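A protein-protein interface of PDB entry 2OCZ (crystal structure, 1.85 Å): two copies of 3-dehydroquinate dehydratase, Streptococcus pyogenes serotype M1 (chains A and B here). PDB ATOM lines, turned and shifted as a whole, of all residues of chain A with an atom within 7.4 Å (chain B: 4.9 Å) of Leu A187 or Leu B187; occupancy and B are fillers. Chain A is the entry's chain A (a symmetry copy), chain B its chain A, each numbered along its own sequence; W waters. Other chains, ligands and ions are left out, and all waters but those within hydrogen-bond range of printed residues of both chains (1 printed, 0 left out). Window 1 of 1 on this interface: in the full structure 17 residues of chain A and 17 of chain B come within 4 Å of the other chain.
The guanidinium group (NE) of Arg B186 sits close to the backbone carbonyl oxygen (O) of Val A224 (3.3 Å).
Among the printed residues, pairs that only touch across the chains: Leu A158 with Met B161 (3.6 Å), Met A161 with Met B161 (3.8 Å), Met A161 with Leu B187 (3.8 Å), Leu A187 with Met B161 (3.8 Å), Leu A187 with Leu B187 (3.9 Å), Leu A187 with Phe B190 (3.8 Å), Leu A187 with Ala B191 (3.6 Å), Leu A187 with Val B194 (3.99 Å), Leu A187 with Leu B225 (3.6 Å), Phe A190 with Leu B187 (3.8 Å), Phe A190 with Leu B225 (3.7 Å), Ala A191 with Leu B187 (3.6 Å), Val A194 with Leu B187 (3.99 Å), Val A224 with Phe B190 (3.5 Å), Leu A225 with Leu B187 (3.6 Å) and Leu A225 with Phe B190 (3.7 Å).
Of the printed residues of chain B, Met A161 touches Met B161 (3.8 Å) and Leu B187 (3.8 Å). Asp A193 touches none of the printed residues of chain B. Ile A221 touches none of the printed residues of chain B. Printed residues of chain A within 4 Å of Leu B187: Met A161, Leu A187, Phe A190, Ala A191, Val A194 and Leu A225. Of the printed residues of chain A, Phe B190 touches Leu A187, Val A224 and Leu A225. Printed residues of chain A within 4 Å of Leu B225: Leu A187 (3.6 Å) and Phe A190 (3.7 Å). The nearest printed residue of chain A that does not touch Leu B187 is Ile A195 (5.6 Å).
Met B161 touches its own counterpart, Met A161. Leu B187 touches its own counterpart, Leu A187. Leu A187 touches Phe B190, and with the chains exchanged Phe A190 touches Leu B187. Leu A187 touches Leu B225, and with the chains exchanged Leu A225 touches Leu B187. Of the 17 pairs that touch across the chains among the printed residues, 14 have their exchanged pair printed and touching as well.
Of the 22 printed residues of chain A, 8 touch a printed residue of chain B. Among the printed residues, 17 pairs touch across the chains. Among the printed residues, no Asp or Glu carboxylate lies within 4 Å of a Lys or Arg side-chain nitrogen of the other chain.
Water W1 bridges the backbone carbonyl oxygen (O) of Lys A183 (2.6 Å) and the backbone carbonyl oxygen (O) of Leu B225 (2.7 Å).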
ATOM      1  N   VAL A 157      -4.416 -24.897 -15.541  1.00  0.00           N
ATOM      2  CA  VAL A 157      -4.124 -24.478 -16.914  1.00  0.00           C
ATOM      3  C   VAL A 157      -2.605 -24.230 -16.980  1.00  0.00           C
ATOM      4  O   VAL A 157      -1.949 -24.684 -17.909  1.00  0.00           O
ATOM      5  CB  VAL A 157      -4.853 -23.164 -17.286  1.00  0.00           C
ATOM      6  CG1 VAL A 157      -4.546 -22.775 -18.719  1.00  0.00           C
ATOM      7  CG2 VAL A 157      -6.383 -23.297 -17.106  1.00  0.00           C
ATOM      8  N   LEU A 158      -2.083 -23.496 -15.998  1.00  0.00           N
ATOM      9  CA  LEU A 158      -0.643 -23.208 -15.925  1.00  0.00           C
ATOM     10  C   LEU A 158       0.162 -24.487 -15.765  1.00  0.00           C
ATOM     11  O   LEU A 158       1.263 -24.602 -16.322  1.00  0.00           O
ATOM     12  CB  LEU A 158      -0.322 -22.238 -14.789  1.00  0.00           C
ATOM     13  CG  LEU A 158      -0.961 -20.839 -14.917  1.00  0.00           C
ATOM     14  CD1 LEU A 158      -0.614 -20.003 -13.683  1.00  0.00           C
ATOM     15  CD2 LEU A 158      -0.479 -20.170 -16.192  1.00  0.00           C
ATOM     16  N   MET A 161       0.695 -26.123 -19.119  1.00  0.00           N
ATOM     17  CA  MET A 161       1.656 -25.322 -19.853  1.00  0.00           C
ATOM     18  C   MET A 161       3.081 -25.560 -19.355  1.00  0.00           C
ATOM     19  O   MET A 161       3.977 -25.760 -20.159  1.00  0.00           O
ATOM     20  CB  MET A 161       1.243 -23.837 -19.749  1.00  0.00           C
ATOM     21  CG  MET A 161      -0.066 -23.626 -20.485  1.00  0.00           C
ATOM     22  SD  MET A 161      -0.764 -21.807 -20.193  1.00  0.00           S
ATOM     23  CE  MET A 161       0.790 -20.755 -20.804  1.00  0.00           C
ATOM     24  N   SER A 180      -5.059 -27.385 -22.542  1.00  0.00           N
ATOM     25  CA  SER A 180      -5.946 -27.367 -21.406  1.00  0.00           C
ATOM     26  C   SER A 180      -7.291 -26.988 -22.003  1.00  0.00           C
ATOM     27  O   SER A 180      -7.433 -25.940 -22.665  1.00  0.00           O
ATOM     28  CB  SER A 180      -5.487 -26.315 -20.400  1.00  0.00           C
ATOM     29  OG  SER A 180      -6.296 -26.321 -19.246  1.00  0.00           O
ATOM     30  N   GLY A 182     -11.688 -26.461 -22.365  1.00  0.00           N
ATOM     31  CA  GLY A 182     -12.701 -25.577 -21.797  1.00  0.00           C
ATOM     32  C   GLY A 182     -12.421 -24.112 -22.024  1.00  0.00           C
ATOM     33  O   GLY A 182     -11.357 -23.721 -22.529  1.00  0.00           O
ATOM     34  N   LYS A 183     -13.384 -23.287 -21.636  1.00  0.00           N
ATOM     35  CA  LYS A 183     -13.194 -21.849 -21.621  1.00  0.00           C
ATOM     36  C   LYS A 183     -12.002 -21.473 -20.732  1.00  0.00           C
ATOM     37  O   LYS A 183     -11.140 -20.687 -21.135  1.00  0.00           O
ATOM     38  CB  LYS A 183     -14.493 -21.162 -21.151  1.00  0.00           C
ATOM     39  CG  LYS A 183     -14.422 -19.650 -21.077  1.00  0.00           C
ATOM     40  CD  LYS A 183     -15.788 -19.013 -20.759  1.00  0.00           C
ATOM     41  CE  LYS A 183     -15.569 -17.735 -19.946  1.00  0.00           C
ATOM     42  NZ  LYS A 183     -16.831 -17.057 -19.477  1.00  0.00           N
ATOM     43  N   LEU A 184     -11.946 -22.052 -19.533  1.00  0.00           N
ATOM     44  CA  LEU A 184     -10.844 -21.826 -18.609  1.00  0.00           C
ATOM     45  C   LEU A 184      -9.457 -22.027 -19.256  1.00  0.00           C
ATOM     46  O   LEU A 184      -8.565 -21.208 -19.079  1.00  0.00           O
ATOM     47  CB  LEU A 184     -11.007 -22.729 -17.368  1.00  0.00           C
ATOM     48  CG  LEU A 184     -10.079 -22.531 -16.168  1.00  0.00           C
ATOM     49  CD1 LEU A 184      -9.876 -21.038 -15.835  1.00  0.00           C
ATOM     50  CD2 LEU A 184     -10.629 -23.297 -14.920  1.00  0.00           C
ATOM     51  N   GLY A 185      -9.301 -23.103 -20.004  1.00  0.00           N
ATOM     52  CA  GLY A 185      -8.006 -23.491 -20.565  1.00  0.00           C
ATOM     53  C   GLY A 185      -7.693 -22.848 -21.905  1.00  0.00           C
ATOM     54  O   GLY A 185      -6.627 -23.074 -22.455  1.00  0.00           O
ATOM     55  N   ARG A 186      -8.594 -22.008 -22.408  1.00  0.00           N
ATOM     56  CA  ARG A 186      -8.475 -21.495 -23.786  1.00  0.00           C
ATOM     57  C   ARG A 186      -7.148 -20.759 -24.076  1.00  0.00           C
ATOM     58  O   ARG A 186      -6.577 -20.922 -25.143  1.00  0.00           O
ATOM     59  CB  ARG A 186      -9.695 -20.645 -24.208  1.00  0.00           C
ATOM     60  CG  ARG A 186      -9.788 -20.582 -25.738  1.00  0.00           C
ATOM     61  CD  ARG A 186     -10.894 -19.707 -26.260  1.00  0.00           C
ATOM     62  NE  ARG A 186     -12.133 -19.917 -25.525  1.00  0.00           N
ATOM     63  CZ  ARG A 186     -13.182 -20.579 -26.000  1.00  0.00           C
ATOM     64  NH1 ARG A 186     -13.150 -21.091 -27.232  1.00  0.00           N
ATOM     65  NH2 ARG A 186     -14.272 -20.711 -25.246  1.00  0.00           N
ATOM     66  N   LEU A 187      -6.668 -19.963 -23.123  1.00  0.00           N
ATOM     67  CA  LEU A 187      -5.318 -19.369 -23.190  1.00  0.00           C
ATOM     68  C   LEU A 187      -4.232 -20.356 -23.664  1.00  0.00           C
ATOM     69  O   LEU A 187      -3.361 -19.986 -24.465  1.00  0.00           O
ATOM     70  CB  LEU A 187      -4.910 -18.778 -21.836  1.00  0.00           C
ATOM     71  CG  LEU A 187      -3.496 -18.161 -21.777  1.00  0.00           C
ATOM     72  CD1 LEU A 187      -3.467 -16.802 -22.469  1.00  0.00           C
ATOM     73  CD2 LEU A 187      -3.010 -18.035 -20.337  1.00  0.00           C
ATOM     74  N   SER A 188      -4.296 -21.605 -23.208  1.00  0.00           N
ATOM     75  CA  SER A 188      -3.283 -22.582 -23.576  1.00  0.00           C
ATOM     76  C   SER A 188      -3.268 -22.848 -25.074  1.00  0.00           C
ATOM     77  O   SER A 188      -2.243 -23.245 -25.611  1.00  0.00           O
ATOM     78  CB  SER A 188      -3.451 -23.920 -22.839  1.00  0.00           C
ATOM     79  OG  SER A 188      -4.601 -24.619 -23.302  1.00  0.00           O
ATOM     80  N   ARG A 189      -4.403 -22.611 -25.739  1.00  0.00           N
ATOM     81  CA  ARG A 189      -4.508 -22.914 -27.165  1.00  0.00           C
ATOM     82  C   ARG A 189      -3.709 -21.934 -28.007  1.00  0.00           C
ATOM     83  O   ARG A 189      -3.372 -22.231 -29.145  1.00  0.00           O
ATOM     84  CB  ARG A 189      -5.988 -22.961 -27.599  1.00  0.00           C
ATOM     85  CG  ARG A 189      -6.762 -24.136 -26.921  1.00  0.00           C
ATOM     86  CD  ARG A 189      -8.180 -24.229 -27.503  1.00  0.00           C
ATOM     87  NE  ARG A 189      -9.059 -25.188 -26.820  1.00  0.00           N
ATOM     88  CZ  ARG A 189      -9.271 -26.437 -27.227  1.00  0.00           C
ATOM     89  NH1 ARG A 189      -8.654 -26.901 -28.319  1.00  0.00           N
ATOM     90  NH2 ARG A 189     -10.111 -27.224 -26.549  1.00  0.00           N
ATOM     91  N   PHE A 190      -3.387 -20.777 -27.442  1.00  0.00           N
ATOM     92  CA  PHE A 190      -2.567 -19.792 -28.135  1.00  0.00           C
ATOM     93  C   PHE A 190      -1.128 -19.738 -27.592  1.00  0.00           C
ATOM     94  O   PHE A 190      -0.346 -18.847 -27.958  1.00  0.00           O
ATOM     95  CB  PHE A 190      -3.212 -18.435 -27.959  1.00  0.00           C
ATOM     96  CG  PHE A 190      -4.683 -18.452 -28.197  1.00  0.00           C
ATOM     97  CD1 PHE A 190      -5.193 -18.914 -29.414  1.00  0.00           C
ATOM     98  CD2 PHE A 190      -5.554 -18.032 -27.203  1.00  0.00           C
ATOM     99  CE1 PHE A 190      -6.579 -18.951 -29.646  1.00  0.00           C
ATOM    100  CE2 PHE A 190      -6.938 -18.067 -27.413  1.00  0.00           C
ATOM    101  CZ  PHE A 190      -7.450 -18.527 -28.630  1.00  0.00           C
ATOM    102  N   ALA A 191      -0.806 -20.667 -26.697  1.00  0.00           N
ATOM    103  CA  ALA A 191       0.492 -20.667 -25.989  1.00  0.00           C
ATOM    104  C   ALA A 191       1.520 -21.640 -26.591  1.00  0.00           C
ATOM    105  O   ALA A 191       2.577 -21.864 -26.004  1.00  0.00           O
ATOM    106  CB  ALA A 191       0.277 -20.991 -24.530  1.00  0.00           C
ATOM    107  N   GLY A 192       1.237 -22.200 -27.763  1.00  0.00           N
ATOM    108  CA  GLY A 192       2.059 -23.293 -28.280  1.00  0.00           C
ATOM    109  C   GLY A 192       3.512 -22.900 -28.482  1.00  0.00           C
ATOM    110  O   GLY A 192       4.418 -23.699 -28.228  1.00  0.00           O
ATOM    111  N   ASP A 193       3.747 -21.663 -28.912  1.00  0.00           N
ATOM    112  CA  ASP A 193       5.107 -21.216 -29.144  1.00  0.00           C
ATOM    113  C   ASP A 193       5.887 -21.079 -27.835  1.00  0.00           C
ATOM    114  O   ASP A 193       7.074 -21.396 -27.788  1.00  0.00           O
ATOM    115  CB  ASP A 193       5.128 -19.894 -29.890  1.00  0.00           C
ATOM    116  CG  ASP A 193       4.895 -20.053 -31.382  1.00  0.00           C
ATOM    117  OD1 ASP A 193       4.957 -21.198 -31.924  1.00  0.00           O
ATOM    118  OD2 ASP A 193       4.635 -19.001 -32.032  1.00  0.00           O
ATOM    119  N   VAL A 194       5.227 -20.610 -26.782  1.00  0.00           N
ATOM    120  CA  VAL A 194       5.879 -20.457 -25.490  1.00  0.00           C
ATOM    121  C   VAL A 194       6.091 -21.822 -24.863  1.00  0.00           C
ATOM    122  O   VAL A 194       7.194 -22.103 -24.368  1.00  0.00           O
ATOM    123  CB  VAL A 194       5.063 -19.534 -24.538  1.00  0.00           C
ATOM    124  CG1 VAL A 194       5.591 -19.597 -23.083  1.00  0.00           C
ATOM    125  CG2 VAL A 194       5.094 -18.076 -25.075  1.00  0.00           C
ATOM    126  N   ILE A 195       5.045 -22.655 -24.863  1.00  0.00           N
ATOM    127  CA  ILE A 195       5.120 -23.945 -24.164  1.00  0.00           C
ATOM    128  C   ILE A 195       5.819 -25.084 -24.903  1.00  0.00           C
ATOM    129  O   ILE A 195       6.199 -26.055 -24.257  1.00  0.00           O
ATOM    130  CB  ILE A 195       3.775 -24.418 -23.582  1.00  0.00           C
ATOM    131  CG1 ILE A 195       2.838 -24.975 -24.668  1.00  0.00           C
ATOM    132  CG2 ILE A 195       3.105 -23.264 -22.757  1.00  0.00           C
ATOM    133  CD1 ILE A 195       1.557 -25.611 -24.057  1.00  0.00           C
ATOM    134  N   GLY A 211     -14.170 -24.086 -25.414  1.00  0.00           N
ATOM    135  CA  GLY A 211     -12.724 -24.127 -25.586  1.00  0.00           C
ATOM    136  C   GLY A 211     -12.186 -24.133 -27.014  1.00  0.00           C
ATOM    137  O   GLY A 211     -11.263 -23.364 -27.321  1.00  0.00           O
ATOM    138  N   ILE A 221      -4.884 -14.624 -33.686  1.00  0.00           N
ATOM    139  CA  ILE A 221      -4.043 -14.662 -32.490  1.00  0.00           C
ATOM    140  C   ILE A 221      -2.575 -14.786 -32.870  1.00  0.00           C
ATOM    141  O   ILE A 221      -1.747 -14.046 -32.332  1.00  0.00           O
ATOM    142  CB  ILE A 221      -4.433 -15.788 -31.502  1.00  0.00           C
ATOM    143  CG1 ILE A 221      -5.950 -15.813 -31.251  1.00  0.00           C
ATOM    144  CG2 ILE A 221      -3.654 -15.634 -30.188  1.00  0.00           C
ATOM    145  CD1 ILE A 221      -6.536 -14.569 -30.578  1.00  0.00           C
ATOM    146  N   VAL A 224      -1.162 -11.363 -33.697  1.00  0.00           N
ATOM    147  CA  VAL A 224      -0.779 -10.531 -32.549  1.00  0.00           C
ATOM    148  C   VAL A 224       0.495 -11.035 -31.837  1.00  0.00           C
ATOM    149  O   VAL A 224       1.360 -10.234 -31.464  1.00  0.00           O
ATOM    150  CB  VAL A 224      -1.950 -10.378 -31.545  1.00  0.00           C
ATOM    151  CG1 VAL A 224      -1.617  -9.335 -30.480  1.00  0.00           C
ATOM    152  CG2 VAL A 224      -3.228  -9.976 -32.274  1.00  0.00           C
ATOM    153  N   LEU A 225       0.618 -12.353 -31.678  1.00  0.00           N
ATOM    154  CA  LEU A 225       1.820 -12.958 -31.080  1.00  0.00           C
ATOM    155  C   LEU A 225       3.000 -13.076 -32.047  1.00  0.00           C
ATOM    156  O   LEU A 225       4.145 -13.263 -31.614  1.00  0.00           O
ATOM    157  CB  LEU A 225       1.508 -14.352 -30.527  1.00  0.00           C
ATOM    158  CG  LEU A 225       0.510 -14.461 -29.382  1.00  0.00           C
ATOM    159  CD1 LEU A 225       0.239 -15.925 -29.099  1.00  0.00           C
ATOM    160  CD2 LEU A 225       1.019 -13.741 -28.139  1.00  0.00           C
ATOM    161  N   MET B 161       4.040 -15.659 -14.885  1.00  0.00           N
ATOM    162  CA  MET B 161       2.644 -16.050 -14.822  1.00  0.00           C
ATOM    163  C   MET B 161       2.350 -16.879 -13.574  1.00  0.00           C
ATOM    164  O   MET B 161       1.380 -16.610 -12.883  1.00  0.00           O
ATOM    165  CB  MET B 161       2.283 -16.804 -16.122  1.00  0.00           C
ATOM    166  CG  MET B 161       2.356 -15.846 -17.296  1.00  0.00           C
ATOM    167  SD  MET B 161       2.136 -16.798 -19.007  1.00  0.00           S
ATOM    168  CE  MET B 161       0.403 -17.681 -18.673  1.00  0.00           C
ATOM    169  N   LEU B 184       8.678 -12.169 -26.837  1.00  0.00           N
ATOM    170  CA  LEU B 184       8.659 -13.418 -26.088  1.00  0.00           C
ATOM    171  C   LEU B 184       7.541 -13.472 -25.025  1.00  0.00           C
ATOM    172  O   LEU B 184       6.831 -14.463 -24.919  1.00  0.00           O
ATOM    173  CB  LEU B 184      10.040 -13.666 -25.447  1.00  0.00           C
ATOM    174  CG  LEU B 184      10.325 -15.010 -24.773  1.00  0.00           C
ATOM    175  CD1 LEU B 184       9.798 -16.197 -25.607  1.00  0.00           C
ATOM    176  CD2 LEU B 184      11.857 -15.171 -24.503  1.00  0.00           C
ATOM    177  N   GLY B 185       7.393 -12.402 -24.265  1.00  0.00           N
ATOM    178  CA  GLY B 185       6.469 -12.366 -23.130  1.00  0.00           C
ATOM    179  C   GLY B 185       5.051 -11.965 -23.497  1.00  0.00           C
ATOM    180  O   GLY B 185       4.186 -11.927 -22.637  1.00  0.00           O
ATOM    181  N   ARG B 186       4.797 -11.713 -24.780  1.00  0.00           N
ATOM    182  CA  ARG B 186       3.512 -11.124 -25.203  1.00  0.00           C
ATOM    183  C   ARG B 186       2.271 -11.942 -24.780  1.00  0.00           C
ATOM    184  O   ARG B 186       1.269 -11.370 -24.380  1.00  0.00           O
ATOM    185  CB  ARG B 186       3.482 -10.794 -26.712  1.00  0.00           C
ATOM    186  CG  ARG B 186       2.400  -9.746 -26.999  1.00  0.00           C
ATOM    187  CD  ARG B 186       2.226  -9.411 -28.455  1.00  0.00           C
ATOM    188  NE  ARG B 186       3.509  -9.243 -29.121  1.00  0.00           N
ATOM    189  CZ  ARG B 186       4.017  -8.070 -29.482  1.00  0.00           C
ATOM    190  NH1 ARG B 186       3.336  -6.946 -29.252  1.00  0.00           N
ATOM    191  NH2 ARG B 186       5.200  -8.026 -30.092  1.00  0.00           N
ATOM    192  N   LEU B 187       2.352 -13.268 -24.867  1.00  0.00           N
ATOM    193  CA  LEU B 187       1.322 -14.164 -24.305  1.00  0.00           C
ATOM    194  C   LEU B 187       0.837 -13.745 -22.903  1.00  0.00           C
ATOM    195  O   LEU B 187      -0.368 -13.799 -22.619  1.00  0.00           O
ATOM    196  CB  LEU B 187       1.821 -15.613 -24.256  1.00  0.00           C
ATOM    197  CG  LEU B 187       0.838 -16.636 -23.650  1.00  0.00           C
ATOM    198  CD1 LEU B 187      -0.277 -16.969 -24.636  1.00  0.00           C
ATOM    199  CD2 LEU B 187       1.564 -17.908 -23.218  1.00  0.00           C
ATOM    200  N   SER B 188       1.752 -13.300 -22.043  1.00  0.00           N
ATOM    201  CA  SER B 188       1.377 -12.927 -20.688  1.00  0.00           C
ATOM    202  C   SER B 188       0.406 -11.756 -20.670  1.00  0.00           C
ATOM    203  O   SER B 188      -0.353 -11.611 -19.721  1.00  0.00           O
ATOM    204  CB  SER B 188       2.590 -12.575 -19.812  1.00  0.00           C
ATOM    205  OG  SER B 188       3.177 -11.344 -20.219  1.00  0.00           O
ATOM    206  N   ARG B 189       0.426 -10.940 -21.727  1.00  0.00           N
ATOM    207  CA  ARG B 189      -0.414  -9.743 -21.761  1.00  0.00           C
ATOM    208  C   ARG B 189      -1.881 -10.093 -21.951  1.00  0.00           C
ATOM    209  O   ARG B 189      -2.750  -9.293 -21.636  1.00  0.00           O
ATOM    210  CB  ARG B 189       0.081  -8.767 -22.848  1.00  0.00           C
ATOM    211  CG  ARG B 189       1.502  -8.203 -22.527  1.00  0.00           C
ATOM    212  CD  ARG B 189       1.878  -7.126 -23.555  1.00  0.00           C
ATOM    213  NE  ARG B 189       3.263  -6.645 -23.456  1.00  0.00           N
ATOM    214  CZ  ARG B 189       3.633  -5.545 -22.804  1.00  0.00           C
ATOM    215  NH1 ARG B 189       2.721  -4.802 -22.169  1.00  0.00           N
ATOM    216  NH2 ARG B 189       4.919  -5.178 -22.795  1.00  0.00           N
ATOM    217  N   PHE B 190      -2.155 -11.295 -22.442  1.00  0.00           N
ATOM    218  CA  PHE B 190      -3.526 -11.759 -22.602  1.00  0.00           C
ATOM    219  C   PHE B 190      -3.926 -12.796 -21.537  1.00  0.00           C
ATOM    220  O   PHE B 190      -4.999 -13.411 -21.622  1.00  0.00           O
ATOM    221  CB  PHE B 190      -3.656 -12.385 -23.974  1.00  0.00           C
ATOM    222  CG  PHE B 190      -3.036 -11.564 -25.051  1.00  0.00           C
ATOM    223  CD1 PHE B 190      -3.439 -10.239 -25.244  1.00  0.00           C
ATOM    224  CD2 PHE B 190      -2.040 -12.101 -25.851  1.00  0.00           C
ATOM    225  CE1 PHE B 190      -2.852  -9.447 -26.247  1.00  0.00           C
ATOM    226  CE2 PHE B 190      -1.438 -11.328 -26.850  1.00  0.00           C
ATOM    227  CZ  PHE B 190      -1.841 -10.003 -27.048  1.00  0.00           C
ATOM    228  N   ALA B 191      -3.041 -13.007 -20.567  1.00  0.00           N
ATOM    229  CA  ALA B 191      -3.221 -14.063 -19.548  1.00  0.00           C
ATOM    230  C   ALA B 191      -3.774 -13.539 -18.212  1.00  0.00           C
ATOM    231  O   ALA B 191      -3.814 -14.276 -17.228  1.00  0.00           O
ATOM    232  CB  ALA B 191      -1.909 -14.775 -19.314  1.00  0.00           C
ATOM    233  N   VAL B 194      -6.341 -15.646 -16.260  1.00  0.00           N
ATOM    234  CA  VAL B 194      -5.823 -16.904 -15.745  1.00  0.00           C
ATOM    235  C   VAL B 194      -4.881 -16.629 -14.588  1.00  0.00           C
ATOM    236  O   VAL B 194      -4.988 -17.290 -13.542  1.00  0.00           O
ATOM    237  CB  VAL B 194      -5.109 -17.731 -16.853  1.00  0.00           C
ATOM    238  CG1 VAL B 194      -4.312 -18.921 -16.261  1.00  0.00           C
ATOM    239  CG2 VAL B 194      -6.157 -18.229 -17.887  1.00  0.00           C
ATOM    240  N   LEU B 225     -11.066 -15.084 -25.787  1.00  0.00           N
ATOM    241  CA  LEU B 225     -11.008 -15.670 -24.437  1.00  0.00           C
ATOM    242  C   LEU B 225     -12.282 -15.463 -23.616  1.00  0.00           C
ATOM    243  O   LEU B 225     -12.497 -16.155 -22.612  1.00  0.00           O
ATOM    244  CB  LEU B 225      -9.826 -15.097 -23.648  1.00  0.00           C
ATOM    245  CG  LEU B 225      -8.420 -15.374 -24.161  1.00  0.00           C
ATOM    246  CD1 LEU B 225      -7.425 -14.594 -23.326  1.00  0.00           C
ATOM    247  CD2 LEU B 225      -8.112 -16.866 -24.141  1.00  0.00           C
HETATM  248  O   HOH W   1     -10.908 -18.106 -21.669  1.00  0.00           O
